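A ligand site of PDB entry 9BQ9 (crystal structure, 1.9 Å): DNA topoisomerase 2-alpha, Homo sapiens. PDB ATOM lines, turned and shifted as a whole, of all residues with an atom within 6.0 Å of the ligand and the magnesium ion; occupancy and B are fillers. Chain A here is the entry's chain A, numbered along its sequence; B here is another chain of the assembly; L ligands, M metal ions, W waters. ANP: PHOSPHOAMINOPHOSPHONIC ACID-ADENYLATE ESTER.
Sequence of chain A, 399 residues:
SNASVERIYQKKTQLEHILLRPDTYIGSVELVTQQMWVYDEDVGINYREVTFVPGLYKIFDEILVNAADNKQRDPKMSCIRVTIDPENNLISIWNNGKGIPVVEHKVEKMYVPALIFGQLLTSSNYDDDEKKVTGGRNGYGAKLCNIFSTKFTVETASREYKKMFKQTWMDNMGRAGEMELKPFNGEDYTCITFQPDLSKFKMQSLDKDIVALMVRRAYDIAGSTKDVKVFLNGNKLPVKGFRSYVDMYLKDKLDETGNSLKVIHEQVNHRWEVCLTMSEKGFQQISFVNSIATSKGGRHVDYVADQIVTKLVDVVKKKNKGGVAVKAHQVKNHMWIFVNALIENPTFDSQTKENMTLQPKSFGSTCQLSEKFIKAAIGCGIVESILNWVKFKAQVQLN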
ATOM      1  N   GLU A  62      26.965 -22.929 -14.989  1.00  0.00           N
ATOM      2  CA  GLU A  62      26.231 -24.086 -15.487  1.00  0.00           C
ATOM      3  C   GLU A  62      25.253 -23.698 -16.589  1.00  0.00           C
ATOM      4  O   GLU A  62      25.145 -24.381 -17.615  1.00  0.00           O
ATOM      5  CB  GLU A  62      25.504 -24.804 -14.351  1.00  0.00           C
ATOM      6  CG  GLU A  62      26.427 -25.482 -13.328  1.00  0.00           C
ATOM      7  CD  GLU A  62      27.042 -26.787 -13.854  1.00  0.00           C
ATOM      8  OE1 GLU A  62      26.874 -27.121 -15.049  1.00  0.00           O
ATOM      9  OE2 GLU A  62      27.710 -27.484 -13.065  1.00  0.00           O
ATOM     10  N   ILE A  63      24.512 -22.598 -16.387  1.00  0.00           N
ATOM     11  CA  ILE A  63      23.554 -22.144 -17.384  1.00  0.00           C
ATOM     12  C   ILE A  63      24.263 -21.599 -18.612  1.00  0.00           C
ATOM     13  O   ILE A  63      23.811 -21.780 -19.748  1.00  0.00           O
ATOM     14  CB  ILE A  63      22.604 -21.108 -16.765  1.00  0.00           C
ATOM     15  CG1 ILE A  63      21.951 -21.665 -15.502  1.00  0.00           C
ATOM     16  CG2 ILE A  63      21.550 -20.689 -17.770  1.00  0.00           C
ATOM     17  CD1 ILE A  63      21.162 -22.942 -15.725  1.00  0.00           C
ATOM     18  N   VAL A  65      27.248 -22.431 -19.846  1.00  0.00           N
ATOM     19  CA  VAL A  65      27.780 -23.532 -20.648  1.00  0.00           C
ATOM     20  C   VAL A  65      26.666 -24.283 -21.351  1.00  0.00           C
ATOM     21  O   VAL A  65      26.815 -24.708 -22.498  1.00  0.00           O
ATOM     22  CB  VAL A  65      28.614 -24.467 -19.745  1.00  0.00           C
ATOM     23  CG1 VAL A  65      28.992 -25.756 -20.485  1.00  0.00           C
ATOM     24  CG2 VAL A  65      29.847 -23.742 -19.256  1.00  0.00           C
ATOM     25  N   ASN A  66      25.520 -24.430 -20.696  1.00  0.00           N
ATOM     26  CA  ASN A  66      24.358 -25.062 -21.336  1.00  0.00           C
ATOM     27  C   ASN A  66      23.977 -24.311 -22.604  1.00  0.00           C
ATOM     28  O   ASN A  66      23.582 -24.927 -23.609  1.00  0.00           O
ATOM     29  CB  ASN A  66      23.176 -25.106 -20.367  1.00  0.00           C
ATOM     30  CG  ASN A  66      23.253 -26.256 -19.397  1.00  0.00           C
ATOM     31  OD1 ASN A  66      24.100 -27.135 -19.516  1.00  0.00           O
ATOM     32  ND2 ASN A  66      22.355 -26.250 -18.412  1.00  0.00           N
ATOM     33  N   ALA A  67      24.033 -22.984 -22.568  1.00  0.00           N
ATOM     34  CA  ALA A  67      23.732 -22.199 -23.762  1.00  0.00           C
ATOM     35  C   ALA A  67      24.735 -22.504 -24.878  1.00  0.00           C
ATOM     36  O   ALA A  67      24.351 -22.749 -26.021  1.00  0.00           O
ATOM     37  CB  ALA A  67      23.705 -20.708 -23.435  1.00  0.00           C
ATOM     38  N   ASP A  69      26.467 -25.163 -25.203  1.00  0.00           N
ATOM     39  CA  ASP A  69      26.226 -26.540 -25.638  1.00  0.00           C
ATOM     40  C   ASP A  69      25.220 -26.608 -26.777  1.00  0.00           C
ATOM     41  O   ASP A  69      25.317 -27.489 -27.634  1.00  0.00           O
ATOM     42  CB  ASP A  69      25.724 -27.367 -24.457  1.00  0.00           C
ATOM     43  CG  ASP A  69      26.827 -27.736 -23.489  1.00  0.00           C
ATOM     44  OD1 ASP A  69      28.019 -27.551 -23.825  1.00  0.00           O
ATOM     45  OD2 ASP A  69      26.500 -28.185 -22.371  1.00  0.00           O
ATOM     46  N   ASN A  70      24.244 -25.706 -26.784  1.00  0.00           N
ATOM     47  CA  ASN A  70      23.228 -25.760 -27.832  1.00  0.00           C
ATOM     48  C   ASN A  70      23.815 -25.481 -29.214  1.00  0.00           C
ATOM     49  O   ASN A  70      23.218 -25.895 -30.213  1.00  0.00           O
ATOM     50  CB  ASN A  70      22.103 -24.780 -27.542  1.00  0.00           C
ATOM     51  CG  ASN A  70      20.805 -25.153 -28.237  1.00  0.00           C
ATOM     52  OD1 ASN A  70      20.322 -26.272 -28.091  1.00  0.00           O
ATOM     53  ND2 ASN A  70      20.258 -24.237 -29.016  1.00  0.00           N
ATOM     54  N   ARG A  73      24.527 -28.752 -30.477  1.00  0.00           N
ATOM     55  CA  ARG A  73      23.263 -29.411 -30.802  1.00  0.00           C
ATOM     56  C   ARG A  73      22.655 -28.854 -32.081  1.00  0.00           C
ATOM     57  O   ARG A  73      22.221 -29.604 -32.957  1.00  0.00           O
ATOM     58  CB  ARG A  73      22.293 -29.259 -29.625  1.00  0.00           C
ATOM     59  CG  ARG A  73      20.875 -29.733 -29.908  1.00  0.00           C
ATOM     60  CD  ARG A  73      20.059 -29.841 -28.621  1.00  0.00           C
ATOM     61  NE  ARG A  73      18.655 -30.125 -28.874  1.00  0.00           N
ATOM     62  CZ  ARG A  73      17.697 -29.197 -28.901  1.00  0.00           C
ATOM     63  NH1 ARG A  73      18.009 -27.929 -28.684  1.00  0.00           N
ATOM     64  NH2 ARG A  73      16.431 -29.541 -29.132  1.00  0.00           N
ATOM     65  N   ASN A  95      19.572 -17.950 -25.565  1.00  0.00           N
ATOM     66  CA  ASN A  95      20.229 -18.473 -26.754  1.00  0.00           C
ATOM     67  C   ASN A  95      19.171 -18.788 -27.815  1.00  0.00           C
ATOM     68  O   ASN A  95      18.044 -19.157 -27.489  1.00  0.00           O
ATOM     69  CB  ASN A  95      21.056 -19.741 -26.465  1.00  0.00           C
ATOM     70  CG  ASN A  95      20.187 -20.961 -26.163  1.00  0.00           C
ATOM     71  OD1 ASN A  95      19.862 -21.239 -25.010  1.00  0.00           O
ATOM     72  ND2 ASN A  95      19.795 -21.675 -27.214  1.00  0.00           N
ATOM     73  N   LYS A  98      17.822 -24.331 -31.952  1.00  0.00           N
ATOM     74  CA  LYS A  98      16.677 -25.176 -31.663  1.00  0.00           C
ATOM     75  C   LYS A  98      16.331 -25.145 -30.185  1.00  0.00           C
ATOM     76  O   LYS A  98      17.201 -25.294 -29.311  1.00  0.00           O
ATOM     77  CB  LYS A  98      16.957 -26.609 -32.124  1.00  0.00           C
ATOM     78  CG  LYS A  98      15.772 -27.554 -31.983  1.00  0.00           C
ATOM     79  CD  LYS A  98      16.046 -28.877 -32.691  1.00  0.00           C
ATOM     80  CE  LYS A  98      14.901 -29.860 -32.474  1.00  0.00           C
ATOM     81  NZ  LYS A  98      13.596 -29.297 -32.928  1.00  0.00           N
ATOM     82  N   GLY A  99      15.051 -24.948 -29.895  1.00  0.00           N
ATOM     83  CA  GLY A  99      14.569 -24.984 -28.538  1.00  0.00           C
ATOM     84  C   GLY A  99      14.395 -26.413 -28.040  1.00  0.00           C
ATOM     85  O   GLY A  99      14.651 -27.389 -28.747  1.00  0.00           O
ATOM     86  N   ILE A 100      13.953 -26.524 -26.800  1.00  0.00           N
ATOM     87  CA  ILE A 100      13.709 -27.824 -26.192  1.00  0.00           C
ATOM     88  C   ILE A 100      12.341 -28.281 -26.673  1.00  0.00           C
ATOM     89  O   ILE A 100      11.406 -27.465 -26.747  1.00  0.00           O
ATOM     90  CB  ILE A 100      13.782 -27.757 -24.662  1.00  0.00           C
ATOM     91  CG1 ILE A 100      15.177 -27.277 -24.242  1.00  0.00           C
ATOM     92  CG2 ILE A 100      13.474 -29.107 -24.052  1.00  0.00           C
ATOM     93  CD1 ILE A 100      15.290 -26.981 -22.785  1.00  0.00           C
ATOM     94  N   ILE A 116      13.781 -31.877 -17.535  1.00  0.00           N
ATOM     95  CA  ILE A 116      15.241 -31.717 -17.517  1.00  0.00           C
ATOM     96  C   ILE A 116      15.698 -30.502 -16.730  1.00  0.00           C
ATOM     97  O   ILE A 116      16.914 -30.309 -16.561  1.00  0.00           O
ATOM     98  CB  ILE A 116      15.784 -31.663 -18.961  1.00  0.00           C
ATOM     99  CG1 ILE A 116      15.269 -30.418 -19.681  1.00  0.00           C
ATOM    100  CG2 ILE A 116      15.368 -32.924 -19.711  1.00  0.00           C
ATOM    101  CD1 ILE A 116      15.585 -30.394 -21.165  1.00  0.00           C
ATOM    102  N   PHE A 117      14.784 -29.680 -16.222  1.00  0.00           N
ATOM    103  CA  PHE A 117      15.161 -28.557 -15.373  1.00  0.00           C
ATOM    104  C   PHE A 117      14.668 -28.685 -13.934  1.00  0.00           C
ATOM    105  O   PHE A 117      15.212 -28.008 -13.056  1.00  0.00           O
ATOM    106  CB  PHE A 117      14.629 -27.232 -15.943  1.00  0.00           C
ATOM    107  CG  PHE A 117      15.420 -26.722 -17.112  1.00  0.00           C
ATOM    108  CD1 PHE A 117      16.534 -25.939 -16.917  1.00  0.00           C
ATOM    109  CD2 PHE A 117      15.049 -27.039 -18.409  1.00  0.00           C
ATOM    110  CE1 PHE A 117      17.269 -25.475 -17.986  1.00  0.00           C
ATOM    111  CE2 PHE A 117      15.785 -26.578 -19.487  1.00  0.00           C
ATOM    112  CZ  PHE A 117      16.898 -25.792 -19.282  1.00  0.00           C
ATOM    113  N   THR A 122      18.817 -35.795 -15.022  1.00  0.00           N
ATOM    114  CA  THR A 122      18.120 -35.765 -16.304  1.00  0.00           C
ATOM    115  C   THR A 122      19.015 -35.084 -17.336  1.00  0.00           C
ATOM    116  O   THR A 122      19.553 -34.011 -17.070  1.00  0.00           O
ATOM    117  CB  THR A 122      16.802 -35.005 -16.164  1.00  0.00           C
ATOM    118  OG1 THR A 122      17.053 -33.723 -15.577  1.00  0.00           O
ATOM    119  CG2 THR A 122      15.833 -35.790 -15.296  1.00  0.00           C
ATOM    120  N   SER A 123      19.168 -35.708 -18.505  1.00  0.00           N
ATOM    121  CA  SER A 123      20.148 -35.230 -19.459  1.00  0.00           C
ATOM    122  C   SER A 123      19.884 -35.841 -20.833  1.00  0.00           C
ATOM    123  O   SER A 123      19.224 -36.875 -20.957  1.00  0.00           O
ATOM    124  CB  SER A 123      21.569 -35.563 -18.990  1.00  0.00           C
ATOM    125  OG  SER A 123      22.556 -35.157 -19.923  1.00  0.00           O
ATOM    126  N   SER A 124      20.410 -35.176 -21.863  1.00  0.00           N
ATOM    127  CA  SER A 124      20.486 -35.753 -23.196  1.00  0.00           C
ATOM    128  C   SER A 124      21.881 -36.289 -23.510  1.00  0.00           C
ATOM    129  O   SER A 124      22.145 -36.692 -24.651  1.00  0.00           O
ATOM    130  CB  SER A 124      20.076 -34.719 -24.249  1.00  0.00           C
ATOM    131  OG  SER A 124      20.959 -33.606 -24.206  1.00  0.00           O
ATOM    132  N   ASN A 125      22.764 -36.295 -22.521  1.00  0.00           N
ATOM    133  CA  ASN A 125      24.159 -36.680 -22.692  1.00  0.00           C
ATOM    134  C   ASN A 125      24.507 -38.000 -21.995  1.00  0.00           C
ATOM    135  O   ASN A 125      25.673 -38.229 -21.672  1.00  0.00           O
ATOM    136  CB  ASN A 125      25.077 -35.566 -22.194  1.00  0.00           C
ATOM    137  CG  ASN A 125      24.971 -34.317 -23.036  1.00  0.00           C
ATOM    138  OD1 ASN A 125      25.376 -34.312 -24.192  1.00  0.00           O
ATOM    139  ND2 ASN A 125      24.462 -33.238 -22.453  1.00  0.00           N
ATOM    140  N   GLY A 135      29.615 -29.656 -23.410  1.00  0.00           N
ATOM    141  CA  GLY A 135      30.117 -29.652 -22.058  1.00  0.00           C
ATOM    142  C   GLY A 135      29.260 -30.437 -21.098  1.00  0.00           C
ATOM    143  O   GLY A 135      29.751 -30.867 -20.054  1.00  0.00           O
ATOM    144  N   GLY A 136      27.978 -30.622 -21.422  1.00  0.00           N
ATOM    145  CA  GLY A 136      27.097 -31.330 -20.508  1.00  0.00           C
ATOM    146  C   GLY A 136      27.421 -32.816 -20.479  1.00  0.00           C
ATOM    147  O   GLY A 136      27.621 -33.458 -21.513  1.00  0.00           O
ATOM    148  N   ARG A 137      27.445 -33.365 -19.270  1.00  0.00           N
ATOM    149  CA  ARG A 137      27.810 -34.771 -19.083  1.00  0.00           C
ATOM    150  C   ARG A 137      26.932 -35.484 -18.058  1.00  0.00           C
ATOM    151  O   ARG A 137      26.549 -36.643 -18.277  1.00  0.00           O
ATOM    152  CB  ARG A 137      29.284 -34.879 -18.683  1.00  0.00           C
ATOM    153  CG  ARG A 137      30.285 -34.373 -19.734  1.00  0.00           C
ATOM    154  CD  ARG A 137      30.282 -35.268 -20.972  1.00  0.00           C
ATOM    155  NE  ARG A 137      30.710 -36.616 -20.647  1.00  0.00           N
ATOM    156  CZ  ARG A 137      30.176 -37.724 -21.161  1.00  0.00           C
ATOM    157  NH1 ARG A 137      29.177 -37.650 -22.032  1.00  0.00           N
ATOM    158  NH2 ARG A 137      30.640 -38.897 -20.787  1.00  0.00           N
ATOM    159  N   ASN A 138      26.584 -34.829 -16.950  1.00  0.00           N
ATOM    160  CA  ASN A 138      26.081 -35.529 -15.769  1.00  0.00           C
ATOM    161  C   ASN A 138      24.586 -35.382 -15.497  1.00  0.00           C
ATOM    162  O   ASN A 138      24.034 -36.174 -14.734  1.00  0.00           O
ATOM    163  CB  ASN A 138      26.838 -35.067 -14.516  1.00  0.00           C
ATOM    164  CG  ASN A 138      28.324 -35.294 -14.634  1.00  0.00           C
ATOM    165  OD1 ASN A 138      28.760 -36.347 -15.107  1.00  0.00           O
ATOM    166  ND2 ASN A 138      29.108 -34.309 -14.231  1.00  0.00           N
ATOM    167  N   GLY A 139      23.930 -34.374 -16.067  1.00  0.00           N
ATOM    168  CA  GLY A 139      22.521 -34.174 -15.795  1.00  0.00           C
ATOM    169  C   GLY A 139      22.221 -33.504 -14.468  1.00  0.00           C
ATOM    170  O   GLY A 139      21.135 -33.715 -13.908  1.00  0.00           O
ATOM    171  N   TYR A 140      23.143 -32.689 -13.961  1.00  0.00           N
ATOM    172  CA  TYR A 140      22.977 -31.943 -12.715  1.00  0.00           C
ATOM    173  C   TYR A 140      22.877 -30.443 -12.929  1.00  0.00           C
ATOM    174  O   TYR A 140      22.040 -29.779 -12.298  1.00  0.00           O
ATOM    175  CB  TYR A 140      24.169 -32.211 -11.778  1.00  0.00           C
ATOM    176  CG  TYR A 140      24.000 -33.323 -10.769  1.00  0.00           C
ATOM    177  CD1 TYR A 140      23.021 -33.253  -9.789  1.00  0.00           C
ATOM    178  CD2 TYR A 140      24.844 -34.428 -10.779  1.00  0.00           C
ATOM    179  CE1 TYR A 140      22.870 -34.269  -8.863  1.00  0.00           C
ATOM    180  CE2 TYR A 140      24.708 -35.447  -9.850  1.00  0.00           C
ATOM    181  CZ  TYR A 140      23.724 -35.353  -8.893  1.00  0.00           C
ATOM    182  OH  TYR A 140      23.568 -36.357  -7.962  1.00  0.00           O
ATOM    183  N   GLY A 141      23.749 -29.891 -13.764  1.00  0.00           N
ATOM    184  CA  GLY A 141      23.978 -28.460 -13.926  1.00  0.00           C
ATOM    185  C   GLY A 141      22.798 -27.529 -13.765  1.00  0.00           C
ATOM    186  O   GLY A 141      22.818 -26.631 -12.911  1.00  0.00           O
ATOM    187  N   ALA A 142      21.779 -27.686 -14.614  1.00  0.00           N
ATOM    188  CA  ALA A 142      20.657 -26.759 -14.575  1.00  0.00           C
ATOM    189  C   ALA A 142      19.864 -26.889 -13.286  1.00  0.00           C
ATOM    190  O   ALA A 142      19.375 -25.894 -12.740  1.00  0.00           O
ATOM    191  CB  ALA A 142      19.756 -26.991 -15.783  1.00  0.00           C
ATOM    192  N   LYS A 143      19.699 -28.125 -12.794  1.00  0.00           N
ATOM    193  CA  LYS A 143      18.983 -28.319 -11.543  1.00  0.00           C
ATOM    194  C   LYS A 143      19.731 -27.709 -10.367  1.00  0.00           C
ATOM    195  O   LYS A 143      19.102 -27.239  -9.414  1.00  0.00           O
ATOM    196  CB  LYS A 143      18.725 -29.806 -11.284  1.00  0.00           C
ATOM    197  CG  LYS A 143      17.491 -30.378 -11.972  1.00  0.00           C
ATOM    198  CD  LYS A 143      17.660 -30.513 -13.494  1.00  0.00           C
ATOM    199  CE  LYS A 143      18.810 -31.445 -13.846  1.00  0.00           C
ATOM    200  NZ  LYS A 143      18.941 -31.648 -15.333  1.00  0.00           N
ATOM    201  N   THR A 156      11.289 -21.780 -23.199  1.00  0.00           N
ATOM    202  CA  THR A 156      11.841 -22.386 -24.400  1.00  0.00           C
ATOM    203  C   THR A 156      10.721 -22.538 -25.419  1.00  0.00           C
ATOM    204  O   THR A 156       9.587 -22.866 -25.056  1.00  0.00           O
ATOM    205  CB  THR A 156      12.524 -23.743 -24.092  1.00  0.00           C
ATOM    206  OG1 THR A 156      13.157 -24.260 -25.265  1.00  0.00           O
ATOM    207  CG2 THR A 156      11.519 -24.758 -23.579  1.00  0.00           C
ATOM    208  N   THR A 190      15.741 -20.376 -26.206  1.00  0.00           N
ATOM    209  CA  THR A 190      15.645 -20.796 -24.806  1.00  0.00           C
ATOM    210  C   THR A 190      16.205 -19.688 -23.926  1.00  0.00           C
ATOM    211  O   THR A 190      17.296 -19.179 -24.186  1.00  0.00           O
ATOM    212  CB  THR A 190      16.394 -22.114 -24.550  1.00  0.00           C
ATOM    213  OG1 THR A 190      15.806 -23.156 -25.342  1.00  0.00           O
ATOM    214  CG2 THR A 190      16.333 -22.504 -23.082  1.00  0.00           C
ATOM    215  N   ILE A 192      16.828 -18.735 -19.784  1.00  0.00           N
ATOM    216  CA  ILE A 192      16.838 -19.118 -18.386  1.00  0.00           C
ATOM    217  C   ILE A 192      17.030 -17.850 -17.560  1.00  0.00           C
ATOM    218  O   ILE A 192      18.050 -17.168 -17.696  1.00  0.00           O
ATOM    219  CB  ILE A 192      17.941 -20.135 -18.081  1.00  0.00           C
ATOM    220  CG1 ILE A 192      17.861 -21.320 -19.050  1.00  0.00           C
ATOM    221  CG2 ILE A 192      17.856 -20.587 -16.633  1.00  0.00           C
ATOM    222  CD1 ILE A 192      16.558 -22.069 -19.011  1.00  0.00           C
ATOM    223  N   GLN A 351      31.727 -32.351 -10.486  1.00  0.00           N
ATOM    224  CA  GLN A 351      30.691 -31.666 -11.242  1.00  0.00           C
ATOM    225  C   GLN A 351      31.134 -30.282 -11.695  1.00  0.00           C
ATOM    226  O   GLN A 351      30.669 -29.793 -12.728  1.00  0.00           O
ATOM    227  CB  GLN A 351      29.412 -31.574 -10.390  1.00  0.00           C
ATOM    228  CG  GLN A 351      28.285 -30.738 -10.993  1.00  0.00           C
ATOM    229  CD  GLN A 351      27.722 -31.349 -12.265  1.00  0.00           C
ATOM    230  OE1 GLN A 351      27.730 -32.564 -12.429  1.00  0.00           O
ATOM    231  NE2 GLN A 351      27.225 -30.503 -13.161  1.00  0.00           N
ATOM    232  N   LYS A 353      33.908 -29.452 -12.921  1.00  0.00           N
ATOM    233  CA  LYS A 353      34.574 -29.655 -14.215  1.00  0.00           C
ATOM    234  C   LYS A 353      35.792 -28.753 -14.376  1.00  0.00           C
ATOM    235  O   LYS A 353      36.014 -28.189 -15.448  1.00  0.00           O
ATOM    236  CB  LYS A 353      33.602 -29.455 -15.367  1.00  0.00           C
ATOM    237  CG  LYS A 353      32.468 -30.465 -15.412  1.00  0.00           C
ATOM    238  CD  LYS A 353      31.493 -30.061 -16.510  1.00  0.00           C
ATOM    239  CE  LYS A 353      30.106 -30.646 -16.301  1.00  0.00           C
ATOM    240  NZ  LYS A 353      29.156 -30.153 -17.357  1.00  0.00           N
ATOM    241  N   TYR B   9      16.052 -37.590 -24.118  1.00  0.00           N
ATOM    242  CA  TYR B   9      16.013 -37.076 -22.754  1.00  0.00           C
ATOM    243  C   TYR B   9      15.694 -38.216 -21.797  1.00  0.00           C
ATOM    244  O   TYR B   9      14.585 -38.765 -21.819  1.00  0.00           O
ATOM    245  CB  TYR B   9      14.981 -35.945 -22.648  1.00  0.00           C
ATOM    246  CG  TYR B   9      15.261 -34.817 -23.606  1.00  0.00           C
ATOM    247  CD1 TYR B   9      16.176 -33.834 -23.283  1.00  0.00           C
ATOM    248  CD2 TYR B   9      14.629 -34.749 -24.841  1.00  0.00           C
ATOM    249  CE1 TYR B   9      16.449 -32.800 -24.144  1.00  0.00           C
ATOM    250  CE2 TYR B   9      14.898 -33.712 -25.716  1.00  0.00           C
ATOM    251  CZ  TYR B   9      15.814 -32.745 -25.353  1.00  0.00           C
ATOM    252  OH  TYR B   9      16.103 -31.699 -26.207  1.00  0.00           O
HETATM  253  PG  ANP L   1      25.795 -31.317 -16.714  1.00  0.00           P
HETATM  254  O1G ANP L   1      25.665 -29.847 -16.952  1.00  0.00           O
HETATM  255  O2G ANP L   1      27.303 -31.734 -16.856  1.00  0.00           O
HETATM  256  O3G ANP L   1      25.250 -31.682 -15.278  1.00  0.00           O
HETATM  257  PB  ANP L   1      23.704 -31.520 -18.655  1.00  0.00           P
HETATM  258  O1B ANP L   1      24.093 -30.237 -19.291  1.00  0.00           O
HETATM  259  O2B ANP L   1      23.198 -32.495 -19.761  1.00  0.00           O
HETATM  260  N3B ANP L   1      24.988 -32.234 -17.875  1.00  0.00           N
HETATM  261  PA  ANP L   1      21.853 -29.898 -17.335  1.00  0.00           P
HETATM  262  O1A ANP L   1      22.851 -28.809 -17.300  1.00  0.00           O
HETATM  263  O2A ANP L   1      21.074 -30.113 -16.029  1.00  0.00           O
HETATM  264  O3A ANP L   1      22.526 -31.310 -17.642  1.00  0.00           O
HETATM  265  O5' ANP L   1      20.844 -29.701 -18.524  1.00  0.00           O
HETATM  266  C5' ANP L   1      19.804 -30.699 -18.704  1.00  0.00           C
HETATM  267  C4' ANP L   1      19.496 -30.850 -20.174  1.00  0.00           C
HETATM  268  O4' ANP L   1      18.685 -29.744 -20.621  1.00  0.00           O
HETATM  269  C3' ANP L   1      20.704 -30.845 -21.100  1.00  0.00           C
HETATM  270  O3' ANP L   1      21.281 -32.143 -21.173  1.00  0.00           O
HETATM  271  C2' ANP L   1      20.096 -30.402 -22.429  1.00  0.00           C
HETATM  272  O2' ANP L   1      19.520 -31.505 -23.105  1.00  0.00           O
HETATM  273  C1' ANP L   1      18.988 -29.443 -21.974  1.00  0.00           C
HETATM  274  N9  ANP L   1      19.336 -28.023 -22.049  1.00  0.00           N
HETATM  275  C8  ANP L   1      19.873 -27.249 -21.049  1.00  0.00           C
HETATM  276  N7  ANP L   1      20.062 -26.004 -21.377  1.00  0.00           N
HETATM  277  C5  ANP L   1      19.618 -25.942 -22.694  1.00  0.00           C
HETATM  278  C6  ANP L   1      19.554 -24.890 -23.621  1.00  0.00           C
HETATM  279  N6  ANP L   1      19.958 -23.635 -23.364  1.00  0.00           N
HETATM  280  N1  ANP L   1      19.050 -25.160 -24.846  1.00  0.00           N
HETATM  281  C2  ANP L   1      18.651 -26.406 -25.117  1.00  0.00           C
HETATM  282  N3  ANP L   1      18.659 -27.483 -24.319  1.00  0.00           N
HETATM  283  C4  ANP L   1      19.161 -27.171 -23.112  1.00  0.00           C
HETATM  284 MG    MG M   1      24.799 -28.574 -18.149  1.00  0.00          MG
HETATM  285  O   HOH W   1      21.204 -22.035 -20.968  1.00  0.00           O
HETATM  286  O   HOH W   2      22.252 -27.493 -23.378  1.00  0.00           O
HETATM  287  O   HOH W   3      26.543 -28.325 -19.350  1.00  0.00           O
HETATM  288  O   HOH W   4      25.279 -26.999 -16.889  1.00  0.00           O
HETATM  289  O   HOH W   5      20.257 -24.174 -19.190  1.00  0.00           O
HETATM  290  O   HOH W   6      24.011 -29.250 -22.081  1.00  0.00           O
HETATM  291  O   HOH W   7      18.234 -30.040 -25.595  1.00  0.00           O
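One residue has an atom within 4 Å of the magnesium ion: Asn 66.
Glu 62 touches the ligand (OE1 to O1G, 3.5 Å).
Asn 70 touches the ligand.
Arg 73 touches the ligand (NH1 to C2, 3.9 Å).
CG1 of Ile 100 touches N3 of the ligand, 3.5 Å away.
Ile 116 touches the ligand (CD1 to O4', 3.2 Å).
CZ of Phe 117 touches C8 of the ligand, 3.8 Å away.
Thr 122 touches the ligand.
Gly 136 touches the ligand (CA to O1B, 3.4 Å).
CG2 of Thr 190 touches N6 of the ligand, at 3.8 Å.
CE1 of Tyr 9 of chain B touches O2' of the ligand, at 3.5 Å.
24 residues have an atom within 4 Å of the ligand: Glu 62, Asn 66, Asn 70, Arg 73, Asn 95, Ile 100, Ile 116, Phe 117, Thr 122, Ser 123, Ser 124, Asn 125, Gly 136, Arg 137, Asn 138, Gly 139, Tyr 140, Gly 141, Ala 142, Lys 143, Thr 190, Gln 351, Lys 353 and Tyr 9 of chain B.
The nearest printed residue that does not touch the ligand is Ala 67 (4.1 Å).
An oxygen (O2A) of the ligand sits at hydrogen-bond distance from the backbone NH (N) of Ala 142, 2.9 Å away.
O2B of the ligand is in hydrogen-bond range of OG of Ser 123, at 2.7 Å.
N of Gly 141 lies within hydrogen-bond range of O3G of the ligand (2.8 Å).
N of Arg 137 lies within hydrogen-bond range of O2G of the ligand.
The backbone NH of Ser 124 sits at hydrogen-bond distance from an oxygen (O3') of the ligand (3.2 Å).
The backbone NH of Gly 139 lies within hydrogen-bond range of an oxygen (O3G) of the ligand, 3.1 Å away.
An oxygen (O2A) of the ligand is in salt-bridge range of the side-chain amino group (NZ) of Lys 143 (2.7 Å).
O2G of the ligand sits at hydrogen-bond distance from N of Asn 138, at 3.2 Å.
NE2 of Gln 351 lies within hydrogen-bond range of O3G of the ligand.
The side-chain hydroxyl (OG) of Ser 124 sits at hydrogen-bond distance from an oxygen (O2') of the ligand (2.8 Å).
N of Tyr 140 is in hydrogen-bond range of O3G of the ligand (2.7 Å).
ND2 of Asn 125 lies within hydrogen-bond range of O2B of the ligand (3.1 Å).
The side-chain amide oxygen (OD1) of Asn 95 lies within hydrogen-bond range of a nitrogen (N6) of the ligand, at 2.9 Å.
The side-chain amino group (NZ) of Lys 353 lies within salt-bridge range of an oxygen (O2G) of the ligand, 2.5 Å away.
The backbone carbonyl oxygen of Asn 95 is in hydrogen-bond range of the backbone NH of Thr 190 (2.9 Å).
The side-chain amide oxygen (OD1) of Asn 70 lies within hydrogen-bond range of the guanidinium group (NH1) of Arg 73 (2.9 Å).
N of Gly 136 sits at hydrogen-bond distance from OD2 of Asp 69.
O of Gly 139 lies within hydrogen-bond range of N of Thr 122 (3.3 Å).
The side-chain amide nitrogen (NE2) of Gln 351 is in hydrogen-bond range of the side-chain carboxylate (OE2) of Glu 62 (3.1 Å).
OG of Ser 123 sits at hydrogen-bond distance from N of Asn 125, 2.8 Å away.
The side-chain amino group of Lys 353 is in hydrogen-bond range of the backbone carbonyl oxygen of Gly 135.
The side-chain amide nitrogen of Asn 125 sits close to the backbone carbonyl oxygen of Gly 136, 3.3 Å away.
The magnesium ion is bound by an oxygen (O1G) of the ligand, water W4, the side-chain amide oxygen of Asn 66, water W3, an oxygen (O1B) of the ligand and an oxygen (O1A) of the ligand.
The magnesium ion has six donor atoms within binding distance.
Water W4 bridges OE1 of Glu 62 (2.4 Å) and ND2 of Asn 66 (3.4 Å).
Water W3 lies within hydrogen-bond range of OD2 of Asp 69 (3.0 Å) and N of Gly 136 (3.4 Å).
Water W5 lies within hydrogen-bond range of N7 of the ligand and ND2 of Asn 66.
Water W7 lies within hydrogen-bond range of the side-chain hydroxyl of Tyr 9 of chain B (2.8 Å), a nitrogen (N3) of the ligand (2.9 Å) and the guanidinium group of Arg 73 (3.3 Å).
Water W2 bridges the backbone carbonyl oxygen (O) of Asn 66 (2.9 Å) and a nitrogen (N7) of the ligand (3.3 Å).
Water W1 lies within hydrogen-bond range of O of Ile 63 (2.9 Å), N6 of the ligand (3.1 Å) and N of Ala 67 (3.4 Å).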
